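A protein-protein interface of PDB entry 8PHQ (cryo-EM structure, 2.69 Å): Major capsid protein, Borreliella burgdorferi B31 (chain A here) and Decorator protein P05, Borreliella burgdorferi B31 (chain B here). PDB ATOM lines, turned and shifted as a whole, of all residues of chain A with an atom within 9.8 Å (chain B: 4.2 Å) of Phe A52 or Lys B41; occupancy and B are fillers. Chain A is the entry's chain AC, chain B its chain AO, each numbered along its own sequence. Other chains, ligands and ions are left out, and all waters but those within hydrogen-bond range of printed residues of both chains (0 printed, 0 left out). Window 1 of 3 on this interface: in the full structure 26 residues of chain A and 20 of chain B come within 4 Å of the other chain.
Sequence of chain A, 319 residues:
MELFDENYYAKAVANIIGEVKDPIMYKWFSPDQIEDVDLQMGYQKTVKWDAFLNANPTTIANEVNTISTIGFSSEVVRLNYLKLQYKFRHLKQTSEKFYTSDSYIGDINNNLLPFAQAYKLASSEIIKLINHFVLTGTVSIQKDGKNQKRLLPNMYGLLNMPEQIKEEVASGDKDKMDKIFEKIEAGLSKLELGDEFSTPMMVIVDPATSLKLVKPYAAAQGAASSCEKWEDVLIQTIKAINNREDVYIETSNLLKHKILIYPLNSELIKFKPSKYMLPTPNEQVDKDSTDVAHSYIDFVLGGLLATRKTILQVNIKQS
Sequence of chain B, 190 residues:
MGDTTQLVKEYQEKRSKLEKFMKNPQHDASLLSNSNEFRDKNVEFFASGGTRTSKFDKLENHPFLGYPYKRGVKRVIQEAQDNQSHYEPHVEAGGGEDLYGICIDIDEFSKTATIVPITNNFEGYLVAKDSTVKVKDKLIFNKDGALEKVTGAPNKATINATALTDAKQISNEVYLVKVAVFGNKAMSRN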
ATOM      1  N   LYS A  48       5.003  20.181  13.017  1.00  0.00           N
ATOM      2  CA  LYS A  48       3.929  19.696  13.871  1.00  0.00           C
ATOM      3  C   LYS A  48       3.721  20.653  15.036  1.00  0.00           C
ATOM      4  O   LYS A  48       4.684  21.118  15.652  1.00  0.00           O
ATOM      5  CB  LYS A  48       4.221  18.288  14.399  1.00  0.00           C
ATOM      6  CG  LYS A  48       3.133  17.741  15.306  1.00  0.00           C
ATOM      7  CD  LYS A  48       3.334  16.269  15.611  1.00  0.00           C
ATOM      8  CE  LYS A  48       2.202  15.736  16.473  1.00  0.00           C
ATOM      9  NZ  LYS A  48       2.289  14.264  16.665  1.00  0.00           N
ATOM     10  N   TRP A  49       2.457  20.931  15.340  1.00  0.00           N
ATOM     11  CA  TRP A  49       2.080  21.859  16.394  1.00  0.00           C
ATOM     12  C   TRP A  49       1.569  21.096  17.609  1.00  0.00           C
ATOM     13  O   TRP A  49       0.998  20.010  17.487  1.00  0.00           O
ATOM     14  CB  TRP A  49       1.006  22.826  15.895  1.00  0.00           C
ATOM     15  CG  TRP A  49       1.540  23.915  15.018  1.00  0.00           C
ATOM     16  CD1 TRP A  49       1.460  23.983  13.659  1.00  0.00           C
ATOM     17  CD2 TRP A  49       2.224  25.100  15.438  1.00  0.00           C
ATOM     18  NE1 TRP A  49       2.055  25.132  13.206  1.00  0.00           N
ATOM     19  CE2 TRP A  49       2.533  25.836  14.278  1.00  0.00           C
ATOM     20  CE3 TRP A  49       2.609  25.608  16.681  1.00  0.00           C
ATOM     21  CZ2 TRP A  49       3.206  27.054  14.325  1.00  0.00           C
ATOM     22  CZ3 TRP A  49       3.277  26.817  16.724  1.00  0.00           C
ATOM     23  CH2 TRP A  49       3.570  27.526  15.555  1.00  0.00           C
ATOM     24  N   ASP A  50       1.770  21.680  18.790  1.00  0.00           N
ATOM     25  CA  ASP A  50       1.406  21.016  20.032  1.00  0.00           C
ATOM     26  C   ASP A  50       1.025  22.070  21.062  1.00  0.00           C
ATOM     27  O   ASP A  50       1.419  23.234  20.957  1.00  0.00           O
ATOM     28  CB  ASP A  50       2.560  20.143  20.539  1.00  0.00           C
ATOM     29  CG  ASP A  50       2.161  19.246  21.690  1.00  0.00           C
ATOM     30  OD1 ASP A  50       0.993  19.307  22.128  1.00  0.00           O
ATOM     31  OD2 ASP A  50       3.022  18.471  22.154  1.00  0.00           O
ATOM     32  N   ALA A  51       0.263  21.648  22.071  1.00  0.00           N
ATOM     33  CA  ALA A  51      -0.183  22.530  23.140  1.00  0.00           C
ATOM     34  C   ALA A  51       0.041  21.862  24.490  1.00  0.00           C
ATOM     35  O   ALA A  51       0.045  20.635  24.600  1.00  0.00           O
ATOM     36  CB  ALA A  51      -1.663  22.898  22.987  1.00  0.00           C
ATOM     37  N   PHE A  52       0.224  22.687  25.519  1.00  0.00           N
ATOM     38  CA  PHE A  52       0.509  22.181  26.853  1.00  0.00           C
ATOM     39  C   PHE A  52      -0.058  23.137  27.893  1.00  0.00           C
ATOM     40  O   PHE A  52      -0.283  24.319  27.624  1.00  0.00           O
ATOM     41  CB  PHE A  52       2.014  21.995  27.087  1.00  0.00           C
ATOM     42  CG  PHE A  52       2.854  23.143  26.602  1.00  0.00           C
ATOM     43  CD1 PHE A  52       3.181  23.273  25.264  1.00  0.00           C
ATOM     44  CD2 PHE A  52       3.313  24.097  27.493  1.00  0.00           C
ATOM     45  CE1 PHE A  52       3.949  24.332  24.825  1.00  0.00           C
ATOM     46  CE2 PHE A  52       4.082  25.158  27.059  1.00  0.00           C
ATOM     47  CZ  PHE A  52       4.400  25.274  25.725  1.00  0.00           C
ATOM     48  N   LEU A  53      -0.269  22.608  29.095  1.00  0.00           N
ATOM     49  CA  LEU A  53      -0.795  23.373  30.218  1.00  0.00           C
ATOM     50  C   LEU A  53       0.357  23.797  31.118  1.00  0.00           C
ATOM     51  O   LEU A  53       1.130  22.953  31.581  1.00  0.00           O
ATOM     52  CB  LEU A  53      -1.806  22.544  31.012  1.00  0.00           C
ATOM     53  CG  LEU A  53      -2.965  21.911  30.241  1.00  0.00           C
ATOM     54  CD1 LEU A  53      -3.902  21.183  31.187  1.00  0.00           C
ATOM     55  CD2 LEU A  53      -3.722  22.956  29.443  1.00  0.00           C
ATOM     56  N   ASN A  54       0.467  25.101  31.370  1.00  0.00           N
ATOM     57  CA  ASN A  54       1.580  25.631  32.147  1.00  0.00           C
ATOM     58  C   ASN A  54       1.340  25.616  33.650  1.00  0.00           C
ATOM     59  O   ASN A  54       2.309  25.694  34.413  1.00  0.00           O
ATOM     60  CB  ASN A  54       1.901  27.063  31.710  1.00  0.00           C
ATOM     61  CG  ASN A  54       2.380  27.141  30.277  1.00  0.00           C
ATOM     62  OD1 ASN A  54       3.380  26.526  29.912  1.00  0.00           O
ATOM     63  ND2 ASN A  54       1.669  27.903  29.456  1.00  0.00           N
ATOM     64  N   ALA A  55       0.093  25.519  34.094  1.00  0.00           N
ATOM     65  CA  ALA A  55      -0.213  25.534  35.518  1.00  0.00           C
ATOM     66  C   ALA A  55      -1.602  24.943  35.723  1.00  0.00           C
ATOM     67  O   ALA A  55      -2.295  24.587  34.767  1.00  0.00           O
ATOM     68  CB  ALA A  55      -0.118  26.950  36.091  1.00  0.00           C
ATOM     69  N   ASN A  56      -1.999  24.838  36.988  1.00  0.00           N
ATOM     70  CA  ASN A  56      -3.357  24.442  37.306  1.00  0.00           C
ATOM     71  C   ASN A  56      -4.332  25.518  36.833  1.00  0.00           C
ATOM     72  O   ASN A  56      -3.974  26.696  36.754  1.00  0.00           O
ATOM     73  CB  ASN A  56      -3.519  24.225  38.809  1.00  0.00           C
ATOM     74  CG  ASN A  56      -2.728  23.039  39.316  1.00  0.00           C
ATOM     75  OD1 ASN A  56      -2.898  21.916  38.845  1.00  0.00           O
ATOM     76  ND2 ASN A  56      -1.867  23.280  40.297  1.00  0.00           N
ATOM     77  N   SER A  68      -4.010  31.447  34.675  1.00  0.00           N
ATOM     78  CA  SER A  68      -3.051  30.486  34.151  1.00  0.00           C
ATOM     79  C   SER A  68      -3.172  30.377  32.636  1.00  0.00           C
ATOM     80  O   SER A  68      -4.251  30.544  32.062  1.00  0.00           O
ATOM     81  CB  SER A  68      -3.268  29.117  34.794  1.00  0.00           C
ATOM     82  OG  SER A  68      -2.993  29.161  36.183  1.00  0.00           O
ATOM     83  N   THR A  69      -2.050  30.083  31.989  1.00  0.00           N
ATOM     84  CA  THR A  69      -1.944  30.132  30.540  1.00  0.00           C
ATOM     85  C   THR A  69      -1.727  28.745  29.950  1.00  0.00           C
ATOM     86  O   THR A  69      -1.208  27.841  30.610  1.00  0.00           O
ATOM     87  CB  THR A  69      -0.799  31.051  30.107  1.00  0.00           C
ATOM     88  OG1 THR A  69       0.436  30.557  30.636  1.00  0.00           O
ATOM     89  CG2 THR A  69      -1.028  32.466  30.611  1.00  0.00           C
ATOM     90  N   ILE A  70      -2.136  28.594  28.693  1.00  0.00           N
ATOM     91  CA  ILE A  70      -1.882  27.398  27.898  1.00  0.00           C
ATOM     92  C   ILE A  70      -0.868  27.767  26.824  1.00  0.00           C
ATOM     93  O   ILE A  70      -1.107  28.680  26.024  1.00  0.00           O
ATOM     94  CB  ILE A  70      -3.168  26.845  27.268  1.00  0.00           C
ATOM     95  CG1 ILE A  70      -4.174  26.449  28.346  1.00  0.00           C
ATOM     96  CG2 ILE A  70      -2.861  25.674  26.352  1.00  0.00           C
ATOM     97  CD1 ILE A  70      -5.482  25.945  27.785  1.00  0.00           C
ATOM     98  N   GLY A  71       0.257  27.059  26.802  1.00  0.00           N
ATOM     99  CA  GLY A  71       1.314  27.341  25.861  1.00  0.00           C
ATOM    100  C   GLY A  71       1.234  26.475  24.619  1.00  0.00           C
ATOM    101  O   GLY A  71       0.602  25.421  24.610  1.00  0.00           O
ATOM    102  N   PHE A  72       1.899  26.934  23.563  1.00  0.00           N
ATOM    103  CA  PHE A  72       1.964  26.209  22.305  1.00  0.00           C
ATOM    104  C   PHE A  72       3.413  26.072  21.868  1.00  0.00           C
ATOM    105  O   PHE A  72       4.267  26.888  22.222  1.00  0.00           O
ATOM    106  CB  PHE A  72       1.166  26.900  21.195  1.00  0.00           C
ATOM    107  CG  PHE A  72      -0.280  27.122  21.528  1.00  0.00           C
ATOM    108  CD1 PHE A  72      -0.670  28.178  22.335  1.00  0.00           C
ATOM    109  CD2 PHE A  72      -1.251  26.267  21.041  1.00  0.00           C
ATOM    110  CE1 PHE A  72      -2.000  28.377  22.639  1.00  0.00           C
ATOM    111  CE2 PHE A  72      -2.580  26.460  21.346  1.00  0.00           C
ATOM    112  CZ  PHE A  72      -2.954  27.516  22.145  1.00  0.00           C
ATOM    113  N   SER A  73       3.680  25.024  21.094  1.00  0.00           N
ATOM    114  CA  SER A  73       5.015  24.756  20.586  1.00  0.00           C
ATOM    115  C   SER A  73       4.926  24.232  19.162  1.00  0.00           C
ATOM    116  O   SER A  73       3.928  23.623  18.766  1.00  0.00           O
ATOM    117  CB  SER A  73       5.763  23.743  21.457  1.00  0.00           C
ATOM    118  OG  SER A  73       5.106  22.489  21.456  1.00  0.00           O
ATOM    119  N   SER A  74       5.982  24.479  18.398  1.00  0.00           N
ATOM    120  CA  SER A  74       6.132  23.945  17.055  1.00  0.00           C
ATOM    121  C   SER A  74       7.426  23.151  16.982  1.00  0.00           C
ATOM    122  O   SER A  74       8.459  23.585  17.500  1.00  0.00           O
ATOM    123  CB  SER A  74       6.149  25.058  16.006  1.00  0.00           C
ATOM    124  OG  SER A  74       7.080  26.066  16.356  1.00  0.00           O
ATOM    125  N   GLU A  75       7.366  21.986  16.350  1.00  0.00           N
ATOM    126  CA  GLU A  75       8.541  21.159  16.139  1.00  0.00           C
ATOM    127  C   GLU A  75       8.711  20.897  14.650  1.00  0.00           C
ATOM    128  O   GLU A  75       7.735  20.651  13.932  1.00  0.00           O
ATOM    129  CB  GLU A  75       8.446  19.836  16.908  1.00  0.00           C
ATOM    130  CG  GLU A  75       7.276  18.955  16.508  1.00  0.00           C
ATOM    131  CD  GLU A  75       7.404  17.543  17.039  1.00  0.00           C
ATOM    132  OE1 GLU A  75       8.416  17.249  17.708  1.00  0.00           O
ATOM    133  OE2 GLU A  75       6.490  16.729  16.791  1.00  0.00           O
ATOM    134  N   ARG A 308       7.174   9.075  18.869  1.00  0.00           N
ATOM    135  CA  ARG A 308       7.808   8.720  20.130  1.00  0.00           C
ATOM    136  C   ARG A 308       7.032   7.618  20.838  1.00  0.00           C
ATOM    137  O   ARG A 308       5.800   7.577  20.796  1.00  0.00           O
ATOM    138  CB  ARG A 308       7.914   9.940  21.044  1.00  0.00           C
ATOM    139  CG  ARG A 308       8.992  10.931  20.653  1.00  0.00           C
ATOM    140  CD  ARG A 308       9.217  11.945  21.760  1.00  0.00           C
ATOM    141  NE  ARG A 308      10.421  12.736  21.544  1.00  0.00           N
ATOM    142  CZ  ARG A 308      10.860  13.673  22.373  1.00  0.00           C
ATOM    143  NH1 ARG A 308      10.216  13.964  23.491  1.00  0.00           N
ATOM    144  NH2 ARG A 308      11.975  14.333  22.074  1.00  0.00           N
ATOM    145  N   SER B  35       1.564  13.263  21.408  1.00  0.00           N
ATOM    146  CA  SER B  35       0.758  14.291  22.055  1.00  0.00           C
ATOM    147  C   SER B  35      -0.461  13.714  22.769  1.00  0.00           C
ATOM    148  O   SER B  35      -1.472  14.400  22.931  1.00  0.00           O
ATOM    149  CB  SER B  35       0.327  15.343  21.035  1.00  0.00           C
ATOM    150  OG  SER B  35      -0.378  14.748  19.959  1.00  0.00           O
ATOM    151  N   GLU B  37      -0.327  12.352  26.006  1.00  0.00           N
ATOM    152  CA  GLU B  37      -0.229  12.720  27.410  1.00  0.00           C
ATOM    153  C   GLU B  37      -0.361  14.230  27.579  1.00  0.00           C
ATOM    154  O   GLU B  37       0.031  15.010  26.707  1.00  0.00           O
ATOM    155  CB  GLU B  37       1.102  12.235  27.990  1.00  0.00           C
ATOM    156  CG  GLU B  37       1.265  12.449  29.487  1.00  0.00           C
ATOM    157  CD  GLU B  37       0.113  11.873  30.287  1.00  0.00           C
ATOM    158  OE1 GLU B  37      -0.120  10.650  30.199  1.00  0.00           O
ATOM    159  OE2 GLU B  37      -0.556  12.642  31.008  1.00  0.00           O
ATOM    160  N   ARG B  39       0.355  15.521  30.975  1.00  0.00           N
ATOM    161  CA  ARG B  39       1.063  15.793  32.215  1.00  0.00           C
ATOM    162  C   ARG B  39       2.565  15.808  31.964  1.00  0.00           C
ATOM    163  O   ARG B  39       3.073  15.026  31.154  1.00  0.00           O
ATOM    164  CB  ARG B  39       0.720  14.749  33.281  1.00  0.00           C
ATOM    165  CG  ARG B  39      -0.692  14.872  33.827  1.00  0.00           C
ATOM    166  CD  ARG B  39      -1.124  13.604  34.542  1.00  0.00           C
ATOM    167  NE  ARG B  39      -1.179  12.459  33.642  1.00  0.00           N
ATOM    168  CZ  ARG B  39      -1.556  11.241  34.006  1.00  0.00           C
ATOM    169  NH1 ARG B  39      -1.922  10.973  35.247  1.00  0.00           N
ATOM    170  NH2 ARG B  39      -1.565  10.267  33.100  1.00  0.00           N
ATOM    171  N   ASP B  40       3.268  16.703  32.662  1.00  0.00           N
ATOM    172  CA  ASP B  40       4.709  16.897  32.494  1.00  0.00           C
ATOM    173  C   ASP B  40       5.043  17.207  31.034  1.00  0.00           C
ATOM    174  O   ASP B  40       5.753  16.467  30.350  1.00  0.00           O
ATOM    175  CB  ASP B  40       5.493  15.682  33.002  1.00  0.00           C
ATOM    176  CG  ASP B  40       5.339  15.477  34.492  1.00  0.00           C
ATOM    177  OD1 ASP B  40       4.662  16.303  35.135  1.00  0.00           O
ATOM    178  OD2 ASP B  40       5.895  14.493  35.022  1.00  0.00           O
ATOM    179  N   LYS B  41       4.507  18.333  30.567  1.00  0.00           N
ATOM    180  CA  LYS B  41       4.576  18.673  29.154  1.00  0.00           C
ATOM    181  C   LYS B  41       4.933  20.140  28.933  1.00  0.00           C
ATOM    182  O   LYS B  41       4.958  20.589  27.781  1.00  0.00           O
ATOM    183  CB  LYS B  41       3.231  18.336  28.492  1.00  0.00           C
ATOM    184  CG  LYS B  41       3.245  18.186  26.985  1.00  0.00           C
ATOM    185  CD  LYS B  41       1.833  17.954  26.476  1.00  0.00           C
ATOM    186  CE  LYS B  41       1.799  17.801  24.971  1.00  0.00           C
ATOM    187  NZ  LYS B  41       0.409  17.636  24.465  1.00  0.00           N
ATOM    188  N   ASN B  42       5.233  20.893  29.992  1.00  0.00           N
ATOM    189  CA  ASN B  42       5.423  22.331  29.893  1.00  0.00           C
ATOM    190  C   ASN B  42       6.786  22.819  30.357  1.00  0.00           C
ATOM    191  O   ASN B  42       7.097  23.997  30.150  1.00  0.00           O
ATOM    192  CB  ASN B  42       4.344  23.066  30.700  1.00  0.00           C
ATOM    193  CG  ASN B  42       4.413  22.752  32.180  1.00  0.00           C
ATOM    194  OD1 ASN B  42       4.253  21.604  32.589  1.00  0.00           O
ATOM    195  ND2 ASN B  42       4.660  23.772  32.991  1.00  0.00           N
ATOM    196  N   VAL B  43       7.602  21.969  30.971  1.00  0.00           N
ATOM    197  CA  VAL B  43       8.915  22.400  31.484  1.00  0.00           C
ATOM    198  C   VAL B  43       9.887  22.265  30.320  1.00  0.00           C
ATOM    199  O   VAL B  43      10.610  21.278  30.167  1.00  0.00           O
ATOM    200  CB  VAL B  43       9.346  21.602  32.717  1.00  0.00           C
ATOM    201  CG1 VAL B  43      10.581  22.228  33.340  1.00  0.00           C
ATOM    202  CG2 VAL B  43       8.212  21.536  33.725  1.00  0.00           C
ATOM    203  N   PHE B  46      11.302  26.373  25.320  1.00  0.00           N
ATOM    204  CA  PHE B  46      10.479  27.127  24.384  1.00  0.00           C
ATOM    205  C   PHE B  46       9.234  27.726  25.026  1.00  0.00           C
ATOM    206  O   PHE B  46       8.479  28.424  24.344  1.00  0.00           O
ATOM    207  CB  PHE B  46      10.095  26.244  23.184  1.00  0.00           C
ATOM    208  CG  PHE B  46       9.341  24.985  23.548  1.00  0.00           C
ATOM    209  CD1 PHE B  46       8.074  25.035  24.109  1.00  0.00           C
ATOM    210  CD2 PHE B  46       9.903  23.743  23.301  1.00  0.00           C
ATOM    211  CE1 PHE B  46       7.396  23.878  24.436  1.00  0.00           C
ATOM    212  CE2 PHE B  46       9.224  22.582  23.620  1.00  0.00           C
ATOM    213  CZ  PHE B  46       7.968  22.651  24.185  1.00  0.00           C
ATOM    214  N   ALA B  47       8.999  27.469  26.313  1.00  0.00           N
ATOM    215  CA  ALA B  47       7.831  28.004  27.011  1.00  0.00           C
ATOM    216  C   ALA B  47       8.105  29.462  27.369  1.00  0.00           C
ATOM    217  O   ALA B  47       8.475  29.808  28.494  1.00  0.00           O
ATOM    218  CB  ALA B  47       7.510  27.170  28.244  1.00  0.00           C
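The backbone carbonyl oxygen (O) of Gly A71 is in hydrogen-bond range of the backbone NH (N) of Phe A52 (2.9 Å). O of Thr A69 is in hydrogen-bond range of ND2 of Asn A54 (3.1 Å). The side-chain amide nitrogen of Asn A54 sits close to the backbone NH of Gly A71, 3.1 Å away. NZ of Lys B41 sits close to O of Glu B37 (3.5 Å). The backbone carbonyl oxygen (O) of Asp A50 lies within hydrogen-bond range of the backbone NH (N) of Ser A73 (2.9 Å).
The side-chain amide nitrogen of Asn B42 is in hydrogen-bond range of the backbone carbonyl oxygen of Asn A54 (3.4 Å). The side-chain amino group of Lys B41 is in hydrogen-bond range of the backbone carbonyl oxygen of Ala A51 (3.0 Å). The side-chain carboxylate (OD1) of Asp A50 lies within salt-bridge range of the side-chain amino group (NZ) of Lys B41.
Of the 18 printed residues of chain A, 6 touch a printed residue of chain B. Hydrophobic or aromatic side chains of chain A within 4 Å of the printed part of chain B: Phe A52. Hydrophobic or aromatic side chains of chain B that line the printed part of chain A: Phe B46. Among the printed residues, Asp or Glu carboxylates within 4 Å of a Lys or Arg side-chain nitrogen of the other chain: Asp A50 with Lys B41 (2.9 Å).
Phe A52 touches just these residues of chain B: Lys B41 (3.3 Å), Asn B42 (3.5 Å) and Phe B46 (3.5 Å). Lys B41 touches just these residues of chain A: Asp A50, Ala A51 and Phe A52. No residue of chain A comes within 4 Å of Ser B35. Printed residues of chain A within 4 Å of Asn B42: Phe A52 (3.5 Å), Leu A53 (3.3 Å) and Asn A54 (3.4 Å). Of the printed residues of chain B, Asp A50 touches Lys B41 (2.9 Å). Printed residues of chain B within 4 Å of Ser A73: Phe B46 (3.4 Å). Printed residues of chain B within 4 Å of Ala A51: Lys B41. Thr A69 touches none of the printed residues of chain B. Arg A308 touches none of the printed residues of chain B. The nearest residue of chain B that does not touch Phe A52 is Ala B47 (4.1 Å). The nearest residue of chain A that does not touch Lys B41 is Leu A53 (5.4 Å).
Lys B41 touches Phe A52. CB of Asn B42 touches CD2 of Phe A52 (3.5 Å). Phe A52 touches Phe B46 (CE1 to CE1, 3.5 Å). Asn B42 touches Leu A53 (CB to O, 3.3 Å). CB of Ser A73 touches CE1 of Phe B46 (3.4 Å).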
